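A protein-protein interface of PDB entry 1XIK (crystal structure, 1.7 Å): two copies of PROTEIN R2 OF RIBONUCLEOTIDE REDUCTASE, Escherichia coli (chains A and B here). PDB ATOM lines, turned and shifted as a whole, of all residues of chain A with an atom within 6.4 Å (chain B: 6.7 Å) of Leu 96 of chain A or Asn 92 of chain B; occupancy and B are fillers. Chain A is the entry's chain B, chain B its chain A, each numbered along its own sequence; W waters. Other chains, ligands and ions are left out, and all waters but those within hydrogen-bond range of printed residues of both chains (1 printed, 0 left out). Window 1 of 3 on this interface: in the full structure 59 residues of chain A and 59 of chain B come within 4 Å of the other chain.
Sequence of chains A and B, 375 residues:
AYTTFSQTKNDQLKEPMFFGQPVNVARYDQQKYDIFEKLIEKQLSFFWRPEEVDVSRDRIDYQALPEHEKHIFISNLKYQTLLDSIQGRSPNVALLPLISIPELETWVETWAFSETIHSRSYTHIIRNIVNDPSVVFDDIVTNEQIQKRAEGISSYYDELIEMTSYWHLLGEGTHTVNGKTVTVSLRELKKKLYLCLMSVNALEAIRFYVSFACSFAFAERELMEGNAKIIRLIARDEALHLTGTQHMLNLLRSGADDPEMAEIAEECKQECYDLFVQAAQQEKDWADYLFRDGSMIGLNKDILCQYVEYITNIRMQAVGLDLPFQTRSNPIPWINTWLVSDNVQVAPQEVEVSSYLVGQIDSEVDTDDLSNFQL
Of the 17 printed residues of chain A, 6 touch a printed residue of chain B.
Hydrophobic or aromatic side chains of chain A that line the printed part of chain B: Tyr 2, Val 93 and Leu 96.
Printed residues of chain B within 4 Å of Tyr 2 of chain A: Arg 89 and Val 93.
Of the printed residues of chain B, Asn 92 of chain A touches Asn 92 (3.6 Å), Leu 96 (3.7 Å) and Glu 109 (3.1 Å).
Printed residues of chain B within 4 Å of Val 93 of chain A: Leu 96.
Printed residues of chain B within 4 Å of Leu 96 of chain A: Asn 92 (3.7 Å) and Val 93 (3.8 Å).
Asn 92 of chain B touches just these residues of chain A: Asn 92 (3.6 Å), Leu 96 (3.7 Å) and Glu 109 (3.0 Å).
Printed residues of chain A within 4 Å of Leu 96 of chain B: Asn 92 and Val 93.
Printed residues of chain A within 4 Å of Glu 109 of chain B: Asn 92.
The nearest residue of chain A that does not touch Asn 92 of chain B is Val 93 of chain A (4.9 Å).
The nearest printed residue of chain B that does not touch Val 93 of chain A is Pro 97 of chain B (4.4 Å).
The backbone carbonyl oxygen (O) of Pro 91 of chain B is in hydrogen-bond range of the backbone NH (N) of Leu 96 of chain B, 3.5 Å away.
OH of Tyr 2 of chain A touches CD of Arg 89 of chain B, at 3.6 Å.
CG2 of Val 93 of chain B touches OH of Tyr 2 of chain A, 3.8 Å away.
Asn 92 of chain B touches Asn 92 of chain A (ND2 to ND2, 3.6 Å).
Leu 96 of chain B touches Asn 92 of chain A.
Val 93 of chain A touches Leu 96 of chain B.
Asn 92 of chain B touches Leu 96 of chain A.
Leu 96 of chain A touches Val 93 of chain B (CB to CG2, 3.8 Å).
Glu 109 of chain A touches Arg 89 of chain B.
Asn 92 of chain B touches its own counterpart, Asn 92 of chain A.
Asn 92 of chain A touches Leu 96 of chain B, and with the chains exchanged Leu 96 of chain A touches Asn 92 of chain B.
Asn 92 of chain A touches Glu 109 of chain B, and with the chains exchanged Glu 109 of chain A touches Asn 92 of chain B.
Val 93 of chain A touches Leu 96 of chain B, and with the chains exchanged Leu 96 of chain A touches Val 93 of chain B.
Water W1 lies within hydrogen-bond range of O of Glu 109 of chain A (3.1 Å), ND2 of Asn 92 of chain A (3.3 Å), O of Glu 109 of chain B (3.4 Å) and ND2 of Asn 92 of chain B (3.4 Å).
The guanidinium group (NH2) of Arg 89 of chain B is in salt-bridge range of the side-chain carboxylate (OE1) of Glu 105 of chain A, at 3.1 Å.
ND2 of Asn 92 of chain A lies within hydrogen-bond range of OE2 of Glu 109 of chain B.
OE1 of Glu 109 of chain A sits close to O of Gly 88 of chain B, 2.7 Å away.
The side-chain amide nitrogen (ND2) of Asn 92 of chain B sits at hydrogen-bond distance from the side-chain carboxylate (OE1) of Glu 109 of chain A (3.0 Å).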
ATOM      1  N   TYR A   2      13.139  16.512  14.996  1.00  0.00           N
ATOM      2  CA  TYR A   2      13.303  15.245  14.320  1.00  0.00           C
ATOM      3  C   TYR A   2      13.927  14.299  15.376  1.00  0.00           C
ATOM      4  O   TYR A   2      14.843  14.703  16.076  1.00  0.00           O
ATOM      5  CB  TYR A   2      14.287  15.299  13.160  1.00  0.00           C
ATOM      6  CG  TYR A   2      14.552  13.872  12.699  1.00  0.00           C
ATOM      7  CD1 TYR A   2      13.559  13.149  11.992  1.00  0.00           C
ATOM      8  CD2 TYR A   2      15.736  13.198  13.029  1.00  0.00           C
ATOM      9  CE1 TYR A   2      13.752  11.816  11.545  1.00  0.00           C
ATOM     10  CE2 TYR A   2      15.923  11.871  12.614  1.00  0.00           C
ATOM     11  CZ  TYR A   2      14.946  11.190  11.849  1.00  0.00           C
ATOM     12  OH  TYR A   2      15.118   9.876  11.438  1.00  0.00           O
ATOM     13  N   SER A  90      20.481  11.634  -2.217  1.00  0.00           N
ATOM     14  CA  SER A  90      19.328  12.463  -1.976  1.00  0.00           C
ATOM     15  C   SER A  90      18.033  11.984  -1.384  1.00  0.00           C
ATOM     16  O   SER A  90      17.400  12.659  -0.574  1.00  0.00           O
ATOM     17  CB  SER A  90      19.131  13.430  -3.134  1.00  0.00           C
ATOM     18  OG  SER A  90      20.434  13.778  -3.562  1.00  0.00           O
ATOM     19  N   PRO A  91      17.583  10.837  -1.835  1.00  0.00           N
ATOM     20  CA  PRO A  91      16.329  10.364  -1.290  1.00  0.00           C
ATOM     21  C   PRO A  91      16.489  10.171   0.250  1.00  0.00           C
ATOM     22  O   PRO A  91      15.567  10.517   1.015  1.00  0.00           O
ATOM     23  CB  PRO A  91      16.147   9.025  -2.001  1.00  0.00           C
ATOM     24  CG  PRO A  91      16.904   9.192  -3.333  1.00  0.00           C
ATOM     25  CD  PRO A  91      18.047  10.063  -3.010  1.00  0.00           C
ATOM     26  N   ASN A  92      17.669   9.685   0.657  1.00  0.00           N
ATOM     27  CA  ASN A  92      18.019   9.483   2.081  1.00  0.00           C
ATOM     28  C   ASN A  92      18.007  10.819   2.820  1.00  0.00           C
ATOM     29  O   ASN A  92      17.214  11.031   3.760  1.00  0.00           O
ATOM     30  CB  ASN A  92      19.393   8.813   2.266  1.00  0.00           C
ATOM     31  CG  ASN A  92      19.321   7.307   2.128  1.00  0.00           C
ATOM     32  OD1 ASN A  92      18.286   6.723   2.335  1.00  0.00           O
ATOM     33  ND2 ASN A  92      20.376   6.690   1.707  1.00  0.00           N
ATOM     34  N   VAL A  93      18.832  11.754   2.379  1.00  0.00           N
ATOM     35  CA  VAL A  93      18.877  13.045   3.049  1.00  0.00           C
ATOM     36  C   VAL A  93      17.618  13.848   3.001  1.00  0.00           C
ATOM     37  O   VAL A  93      17.250  14.525   3.978  1.00  0.00           O
ATOM     38  CB  VAL A  93      20.009  13.909   2.488  1.00  0.00           C
ATOM     39  CG1 VAL A  93      20.017  15.253   3.177  1.00  0.00           C
ATOM     40  CG2 VAL A  93      21.310  13.213   2.726  1.00  0.00           C
ATOM     41  N   ALA A  94      16.945  13.763   1.853  1.00  0.00           N
ATOM     42  CA  ALA A  94      15.746  14.545   1.666  1.00  0.00           C
ATOM     43  C   ALA A  94      14.493  13.941   2.246  1.00  0.00           C
ATOM     44  O   ALA A  94      13.653  14.637   2.827  1.00  0.00           O
ATOM     45  CB  ALA A  94      15.568  14.834   0.145  1.00  0.00           C
ATOM     46  N   LEU A  95      14.312  12.643   2.075  1.00  0.00           N
ATOM     47  CA  LEU A  95      13.057  12.073   2.531  1.00  0.00           C
ATOM     48  C   LEU A  95      13.027  11.429   3.881  1.00  0.00           C
ATOM     49  O   LEU A  95      12.018  11.519   4.575  1.00  0.00           O
ATOM     50  CB  LEU A  95      12.559  11.038   1.524  1.00  0.00           C
ATOM     51  CG  LEU A  95      12.446  11.650   0.127  1.00  0.00           C
ATOM     52  CD1 LEU A  95      11.910  10.615  -0.879  1.00  0.00           C
ATOM     53  CD2 LEU A  95      11.388  12.671   0.354  1.00  0.00           C
ATOM     54  N   LEU A  96      14.098  10.725   4.232  1.00  0.00           N
ATOM     55  CA  LEU A  96      14.127  10.054   5.539  1.00  0.00           C
ATOM     56  C   LEU A  96      13.688  10.920   6.715  1.00  0.00           C
ATOM     57  O   LEU A  96      12.956  10.438   7.557  1.00  0.00           O
ATOM     58  CB  LEU A  96      15.530   9.478   5.830  1.00  0.00           C
ATOM     59  CG  LEU A  96      15.897   8.140   5.174  1.00  0.00           C
ATOM     60  CD1 LEU A  96      17.317   7.641   5.525  1.00  0.00           C
ATOM     61  CD2 LEU A  96      14.793   7.081   5.416  1.00  0.00           C
ATOM     62  N   PRO A  97      14.062  12.197   6.771  1.00  0.00           N
ATOM     63  CA  PRO A  97      13.640  12.978   7.931  1.00  0.00           C
ATOM     64  C   PRO A  97      12.158  13.289   7.920  1.00  0.00           C
ATOM     65  O   PRO A  97      11.624  13.843   8.883  1.00  0.00           O
ATOM     66  CB  PRO A  97      14.414  14.291   7.784  1.00  0.00           C
ATOM     67  CG  PRO A  97      15.519  13.991   6.798  1.00  0.00           C
ATOM     68  CD  PRO A  97      14.990  12.948   5.903  1.00  0.00           C
ATOM     69  N   LEU A  98      11.461  12.977   6.824  1.00  0.00           N
ATOM     70  CA  LEU A  98      10.022  13.326   6.754  1.00  0.00           C
ATOM     71  C   LEU A  98       9.051  12.163   6.701  1.00  0.00           C
ATOM     72  O   LEU A  98       7.842  12.390   6.792  1.00  0.00           O
ATOM     73  CB  LEU A  98       9.741  14.206   5.519  1.00  0.00           C
ATOM     74  CG  LEU A  98      10.452  15.561   5.368  1.00  0.00           C
ATOM     75  CD1 LEU A  98      10.088  16.171   3.984  1.00  0.00           C
ATOM     76  CD2 LEU A  98      10.006  16.511   6.478  1.00  0.00           C
ATOM     77  N   ILE A  99       9.567  10.944   6.522  1.00  0.00           N
ATOM     78  CA  ILE A  99       8.766   9.715   6.435  1.00  0.00           C
ATOM     79  C   ILE A  99       8.183   9.251   7.779  1.00  0.00           C
ATOM     80  O   ILE A  99       8.882   9.179   8.802  1.00  0.00           O
ATOM     81  CB  ILE A  99       9.551   8.594   5.755  1.00  0.00           C
ATOM     82  CG1 ILE A  99       9.833   8.965   4.297  1.00  0.00           C
ATOM     83  CG2 ILE A  99       8.842   7.275   5.897  1.00  0.00           C
ATOM     84  CD1 ILE A  99      10.842   8.009   3.636  1.00  0.00           C
ATOM     85  N   SER A 100       6.895   8.894   7.773  1.00  0.00           N
ATOM     86  CA  SER A 100       6.227   8.449   8.980  1.00  0.00           C
ATOM     87  C   SER A 100       5.689   7.052   9.032  1.00  0.00           C
ATOM     88  O   SER A 100       5.033   6.714  10.016  1.00  0.00           O
ATOM     89  CB  SER A 100       5.210   9.448   9.495  1.00  0.00           C
ATOM     90  OG  SER A 100       4.606  10.158   8.436  1.00  0.00           O
ATOM     91  N   LEU A 104       7.795   2.625   3.780  1.00  0.00           N
ATOM     92  CA  LEU A 104       8.257   3.673   2.891  1.00  0.00           C
ATOM     93  C   LEU A 104       9.676   4.070   3.294  1.00  0.00           C
ATOM     94  O   LEU A 104      10.543   4.311   2.441  1.00  0.00           O
ATOM     95  CB  LEU A 104       7.279   4.819   3.058  1.00  0.00           C
ATOM     96  CG  LEU A 104       7.644   6.028   2.203  1.00  0.00           C
ATOM     97  CD1 LEU A 104       8.116   5.631   0.796  1.00  0.00           C
ATOM     98  CD2 LEU A 104       6.574   7.084   2.256  1.00  0.00           C
ATOM     99  N   GLU A 105       9.945   4.065   4.605  1.00  0.00           N
ATOM    100  CA  GLU A 105      11.282   4.446   5.004  1.00  0.00           C
ATOM    101  C   GLU A 105      12.303   3.452   4.474  1.00  0.00           C
ATOM    102  O   GLU A 105      13.352   3.809   3.955  1.00  0.00           O
ATOM    103  CB  GLU A 105      11.363   4.524   6.536  1.00  0.00           C
ATOM    104  CG  GLU A 105      12.639   5.174   7.017  1.00  0.00           C
ATOM    105  CD  GLU A 105      12.690   5.238   8.541  1.00  0.00           C
ATOM    106  OE1 GLU A 105      12.789   4.126   9.150  1.00  0.00           O
ATOM    107  OE2 GLU A 105      12.639   6.380   9.075  1.00  0.00           O
ATOM    108  N   THR A 106      11.973   2.181   4.599  1.00  0.00           N
ATOM    109  CA  THR A 106      12.899   1.148   4.166  1.00  0.00           C
ATOM    110  C   THR A 106      12.964   1.097   2.659  1.00  0.00           C
ATOM    111  O   THR A 106      14.014   0.790   2.094  1.00  0.00           O
ATOM    112  CB  THR A 106      12.528  -0.220   4.760  1.00  0.00           C
ATOM    113  OG1 THR A 106      12.686  -0.138   6.181  1.00  0.00           O
ATOM    114  CG2 THR A 106      13.463  -1.317   4.332  1.00  0.00           C
ATOM    115  N   VAL A 108      12.815   3.709   0.661  1.00  0.00           N
ATOM    116  CA  VAL A 108      13.679   4.826   0.296  1.00  0.00           C
ATOM    117  C   VAL A 108      15.128   4.483   0.496  1.00  0.00           C
ATOM    118  O   VAL A 108      15.989   4.789  -0.330  1.00  0.00           O
ATOM    119  CB  VAL A 108      13.268   6.059   1.060  1.00  0.00           C
ATOM    120  CG1 VAL A 108      14.432   7.067   1.168  1.00  0.00           C
ATOM    121  CG2 VAL A 108      11.950   6.615   0.456  1.00  0.00           C
ATOM    122  N   GLU A 109      15.412   3.762   1.582  1.00  0.00           N
ATOM    123  CA  GLU A 109      16.788   3.349   1.827  1.00  0.00           C
ATOM    124  C   GLU A 109      17.262   2.300   0.870  1.00  0.00           C
ATOM    125  O   GLU A 109      18.415   2.290   0.512  1.00  0.00           O
ATOM    126  CB  GLU A 109      16.936   2.857   3.263  1.00  0.00           C
ATOM    127  CG  GLU A 109      16.387   3.893   4.174  1.00  0.00           C
ATOM    128  CD  GLU A 109      16.945   3.723   5.546  1.00  0.00           C
ATOM    129  OE1 GLU A 109      18.155   3.934   5.788  1.00  0.00           O
ATOM    130  OE2 GLU A 109      16.141   3.298   6.383  1.00  0.00           O
ATOM    131  N   GLN B  87      19.772   1.883  13.723  1.00  0.00           N
ATOM    132  CA  GLN B  87      20.973   1.880  12.933  1.00  0.00           C
ATOM    133  C   GLN B  87      20.636   1.838  11.444  1.00  0.00           C
ATOM    134  O   GLN B  87      21.481   2.058  10.593  1.00  0.00           O
ATOM    135  CB  GLN B  87      21.761   0.643  13.295  1.00  0.00           C
ATOM    136  CG  GLN B  87      22.536   0.837  14.598  1.00  0.00           C
ATOM    137  CD  GLN B  87      23.302   2.110  14.556  1.00  0.00           C
ATOM    138  OE1 GLN B  87      24.406   2.130  14.060  1.00  0.00           O
ATOM    139  NE2 GLN B  87      22.717   3.185  15.022  1.00  0.00           N
ATOM    140  N   GLY B  88      19.393   1.510  11.133  1.00  0.00           N
ATOM    141  CA  GLY B  88      18.982   1.467   9.725  1.00  0.00           C
ATOM    142  C   GLY B  88      18.807   2.898   9.258  1.00  0.00           C
ATOM    143  O   GLY B  88      19.187   3.167   8.153  1.00  0.00           O
ATOM    144  N   ARG B  89      18.256   3.820  10.042  1.00  0.00           N
ATOM    145  CA  ARG B  89      18.072   5.186   9.557  1.00  0.00           C
ATOM    146  C   ARG B  89      19.130   6.178   9.964  1.00  0.00           C
ATOM    147  O   ARG B  89      19.466   7.129   9.233  1.00  0.00           O
ATOM    148  CB  ARG B  89      16.732   5.724  10.053  1.00  0.00           C
ATOM    149  CG  ARG B  89      16.627   5.866  11.577  1.00  0.00           C
ATOM    150  CD  ARG B  89      15.244   6.333  12.042  1.00  0.00           C
ATOM    151  NE  ARG B  89      14.292   5.254  11.733  1.00  0.00           N
ATOM    152  CZ  ARG B  89      13.803   4.339  12.579  1.00  0.00           C
ATOM    153  NH1 ARG B  89      14.075   4.341  13.886  1.00  0.00           N
ATOM    154  NH2 ARG B  89      12.980   3.394  12.131  1.00  0.00           N
ATOM    155  N   SER B  90      19.622   5.983  11.195  1.00  0.00           N
ATOM    156  CA  SER B  90      20.551   6.955  11.769  1.00  0.00           C
ATOM    157  C   SER B  90      21.823   7.365  11.064  1.00  0.00           C
ATOM    158  O   SER B  90      22.116   8.546  10.892  1.00  0.00           O
ATOM    159  CB  SER B  90      20.621   6.799  13.300  1.00  0.00           C
ATOM    160  OG  SER B  90      19.316   6.590  13.812  1.00  0.00           O
ATOM    161  N   PRO B  91      22.589   6.387  10.633  1.00  0.00           N
ATOM    162  CA  PRO B  91      23.832   6.709   9.933  1.00  0.00           C
ATOM    163  C   PRO B  91      23.538   7.564   8.691  1.00  0.00           C
ATOM    164  O   PRO B  91      24.259   8.517   8.374  1.00  0.00           O
ATOM    165  CB  PRO B  91      24.405   5.351   9.579  1.00  0.00           C
ATOM    166  CG  PRO B  91      23.846   4.423  10.663  1.00  0.00           C
ATOM    167  CD  PRO B  91      22.449   4.942  10.912  1.00  0.00           C
ATOM    168  N   ASN B  92      22.418   7.287   8.050  1.00  0.00           N
ATOM    169  CA  ASN B  92      22.098   8.109   6.897  1.00  0.00           C
ATOM    170  C   ASN B  92      21.626   9.483   7.288  1.00  0.00           C
ATOM    171  O   ASN B  92      22.058  10.483   6.712  1.00  0.00           O
ATOM    172  CB  ASN B  92      20.984   7.437   6.103  1.00  0.00           C
ATOM    173  CG  ASN B  92      21.504   6.311   5.283  1.00  0.00           C
ATOM    174  OD1 ASN B  92      22.662   6.304   4.905  1.00  0.00           O
ATOM    175  ND2 ASN B  92      20.689   5.318   5.057  1.00  0.00           N
ATOM    176  N   VAL B  93      20.711   9.560   8.237  1.00  0.00           N
ATOM    177  CA  VAL B  93      20.262  10.888   8.583  1.00  0.00           C
ATOM    178  C   VAL B  93      21.314  11.755   9.288  1.00  0.00           C
ATOM    179  O   VAL B  93      21.411  12.963   9.048  1.00  0.00           O
ATOM    180  CB  VAL B  93      19.015  10.842   9.493  1.00  0.00           C
ATOM    181  CG1 VAL B  93      18.624  12.276   9.807  1.00  0.00           C
ATOM    182  CG2 VAL B  93      17.848  10.212   8.760  1.00  0.00           C
ATOM    183  N   ALA B  94      22.099  11.138  10.168  1.00  0.00           N
ATOM    184  CA  ALA B  94      23.118  11.868  10.923  1.00  0.00           C
ATOM    185  C   ALA B  94      24.455  12.119  10.248  1.00  0.00           C
ATOM    186  O   ALA B  94      25.054  13.192  10.411  1.00  0.00           O
ATOM    187  CB  ALA B  94      23.359  11.141  12.299  1.00  0.00           C
ATOM    188  N   LEU B  95      24.927  11.126   9.506  1.00  0.00           N
ATOM    189  CA  LEU B  95      26.214  11.233   8.840  1.00  0.00           C
ATOM    190  C   LEU B  95      26.308  11.724   7.408  1.00  0.00           C
ATOM    191  O   LEU B  95      27.250  12.440   7.060  1.00  0.00           O
ATOM    192  CB  LEU B  95      26.973   9.905   8.932  1.00  0.00           C
ATOM    193  CG  LEU B  95      27.153   9.329  10.348  1.00  0.00           C
ATOM    194  CD1 LEU B  95      28.078   8.107  10.405  1.00  0.00           C
ATOM    195  CD2 LEU B  95      27.751  10.482  11.150  1.00  0.00           C
ATOM    196  N   LEU B  96      25.395  11.258   6.563  1.00  0.00           N
ATOM    197  CA  LEU B  96      25.479  11.678   5.165  1.00  0.00           C
ATOM    198  C   LEU B  96      25.623  13.154   4.930  1.00  0.00           C
ATOM    199  O   LEU B  96      26.416  13.556   4.118  1.00  0.00           O
ATOM    200  CB  LEU B  96      24.273  11.195   4.331  1.00  0.00           C
ATOM    201  CG  LEU B  96      24.248   9.764   3.839  1.00  0.00           C
ATOM    202  CD1 LEU B  96      22.883   9.444   3.168  1.00  0.00           C
ATOM    203  CD2 LEU B  96      25.466   9.405   2.996  1.00  0.00           C
ATOM    204  N   PRO B  97      24.892  13.983   5.654  1.00  0.00           N
ATOM    205  CA  PRO B  97      24.992  15.428   5.408  1.00  0.00           C
ATOM    206  C   PRO B  97      26.332  16.045   5.813  1.00  0.00           C
ATOM    207  O   PRO B  97      26.568  17.225   5.546  1.00  0.00           O
ATOM    208  CB  PRO B  97      23.864  16.001   6.265  1.00  0.00           C
ATOM    209  CG  PRO B  97      22.921  14.844   6.479  1.00  0.00           C
ATOM    210  CD  PRO B  97      23.808  13.630   6.588  1.00  0.00           C
ATOM    211  N   GLU B 105      31.096   8.051   2.072  1.00  0.00           N
ATOM    212  CA  GLU B 105      29.660   8.286   1.890  1.00  0.00           C
ATOM    213  C   GLU B 105      28.950   6.985   1.508  1.00  0.00           C
ATOM    214  O   GLU B 105      27.915   6.619   2.077  1.00  0.00           O
ATOM    215  CB  GLU B 105      29.440   9.383   0.815  1.00  0.00           C
ATOM    216  CG  GLU B 105      28.022   9.755   0.667  1.00  0.00           C
ATOM    217  CD  GLU B 105      27.783  10.544  -0.624  1.00  0.00           C
ATOM    218  OE1 GLU B 105      28.062  10.041  -1.738  1.00  0.00           O
ATOM    219  OE2 GLU B 105      27.297  11.682  -0.502  1.00  0.00           O
ATOM    220  N   VAL B 108      28.725   4.316   4.388  1.00  0.00           N
ATOM    221  CA  VAL B 108      27.675   4.583   5.338  1.00  0.00           C
ATOM    222  C   VAL B 108      26.313   4.124   4.818  1.00  0.00           C
ATOM    223  O   VAL B 108      25.493   3.509   5.527  1.00  0.00           O
ATOM    224  CB  VAL B 108      27.713   6.064   5.790  1.00  0.00           C
ATOM    225  CG1 VAL B 108      26.367   6.522   6.343  1.00  0.00           C
ATOM    226  CG2 VAL B 108      28.852   6.242   6.849  1.00  0.00           C
ATOM    227  N   GLU B 109      26.089   4.428   3.540  1.00  0.00           N
ATOM    228  CA  GLU B 109      24.850   4.004   2.920  1.00  0.00           C
ATOM    229  C   GLU B 109      24.796   2.484   2.860  1.00  0.00           C
ATOM    230  O   GLU B 109      23.733   1.921   3.054  1.00  0.00           O
ATOM    231  CB  GLU B 109      24.700   4.677   1.536  1.00  0.00           C
ATOM    232  CG  GLU B 109      24.464   6.191   1.713  1.00  0.00           C
ATOM    233  CD  GLU B 109      24.170   6.886   0.417  1.00  0.00           C
ATOM    234  OE1 GLU B 109      25.097   6.999  -0.412  1.00  0.00           O
ATOM    235  OE2 GLU B 109      22.997   7.264   0.223  1.00  0.00           O
ATOM    236  N   THR B 110      25.895   1.794   2.599  1.00  0.00           N
ATOM    237  CA  THR B 110      25.853   0.334   2.517  1.00  0.00           C
ATOM    238  C   THR B 110      25.639  -0.217   3.920  1.00  0.00           C
ATOM    239  O   THR B 110      24.782  -1.064   4.164  1.00  0.00           O
ATOM    240  CB  THR B 110      27.165  -0.132   1.971  1.00  0.00           C
ATOM    241  OG1 THR B 110      27.313   0.452   0.665  1.00  0.00           O
ATOM    242  CG2 THR B 110      27.187  -1.613   1.815  1.00  0.00           C
ATOM    243  N   ALA B 112      24.279   1.269   6.561  1.00  0.00           N
ATOM    244  CA  ALA B 112      22.886   1.453   6.946  1.00  0.00           C
ATOM    245  C   ALA B 112      21.957   0.477   6.220  1.00  0.00           C
ATOM    246  O   ALA B 112      21.021  -0.082   6.793  1.00  0.00           O
ATOM    247  CB  ALA B 112      22.419   2.883   6.721  1.00  0.00           C
ATOM    248  N   PHE B 113      22.176   0.266   4.934  1.00  0.00           N
ATOM    249  CA  PHE B 113      21.278  -0.630   4.224  1.00  0.00           C
ATOM    250  C   PHE B 113      21.352  -2.029   4.824  1.00  0.00           C
ATOM    251  O   PHE B 113      20.339  -2.718   4.998  1.00  0.00           O
ATOM    252  CB  PHE B 113      21.770  -0.741   2.773  1.00  0.00           C
ATOM    253  CG  PHE B 113      21.100  -1.844   2.055  1.00  0.00           C
ATOM    254  CD1 PHE B 113      19.730  -1.791   1.841  1.00  0.00           C
ATOM    255  CD2 PHE B 113      21.808  -2.931   1.661  1.00  0.00           C
ATOM    256  CE1 PHE B 113      19.060  -2.808   1.218  1.00  0.00           C
ATOM    257  CE2 PHE B 113      21.170  -3.969   1.057  1.00  0.00           C
ATOM    258  CZ  PHE B 113      19.790  -3.896   0.842  1.00  0.00           C
HETATM  259  O   HOH W   1      20.800   3.465   2.152  1.00  0.00           O
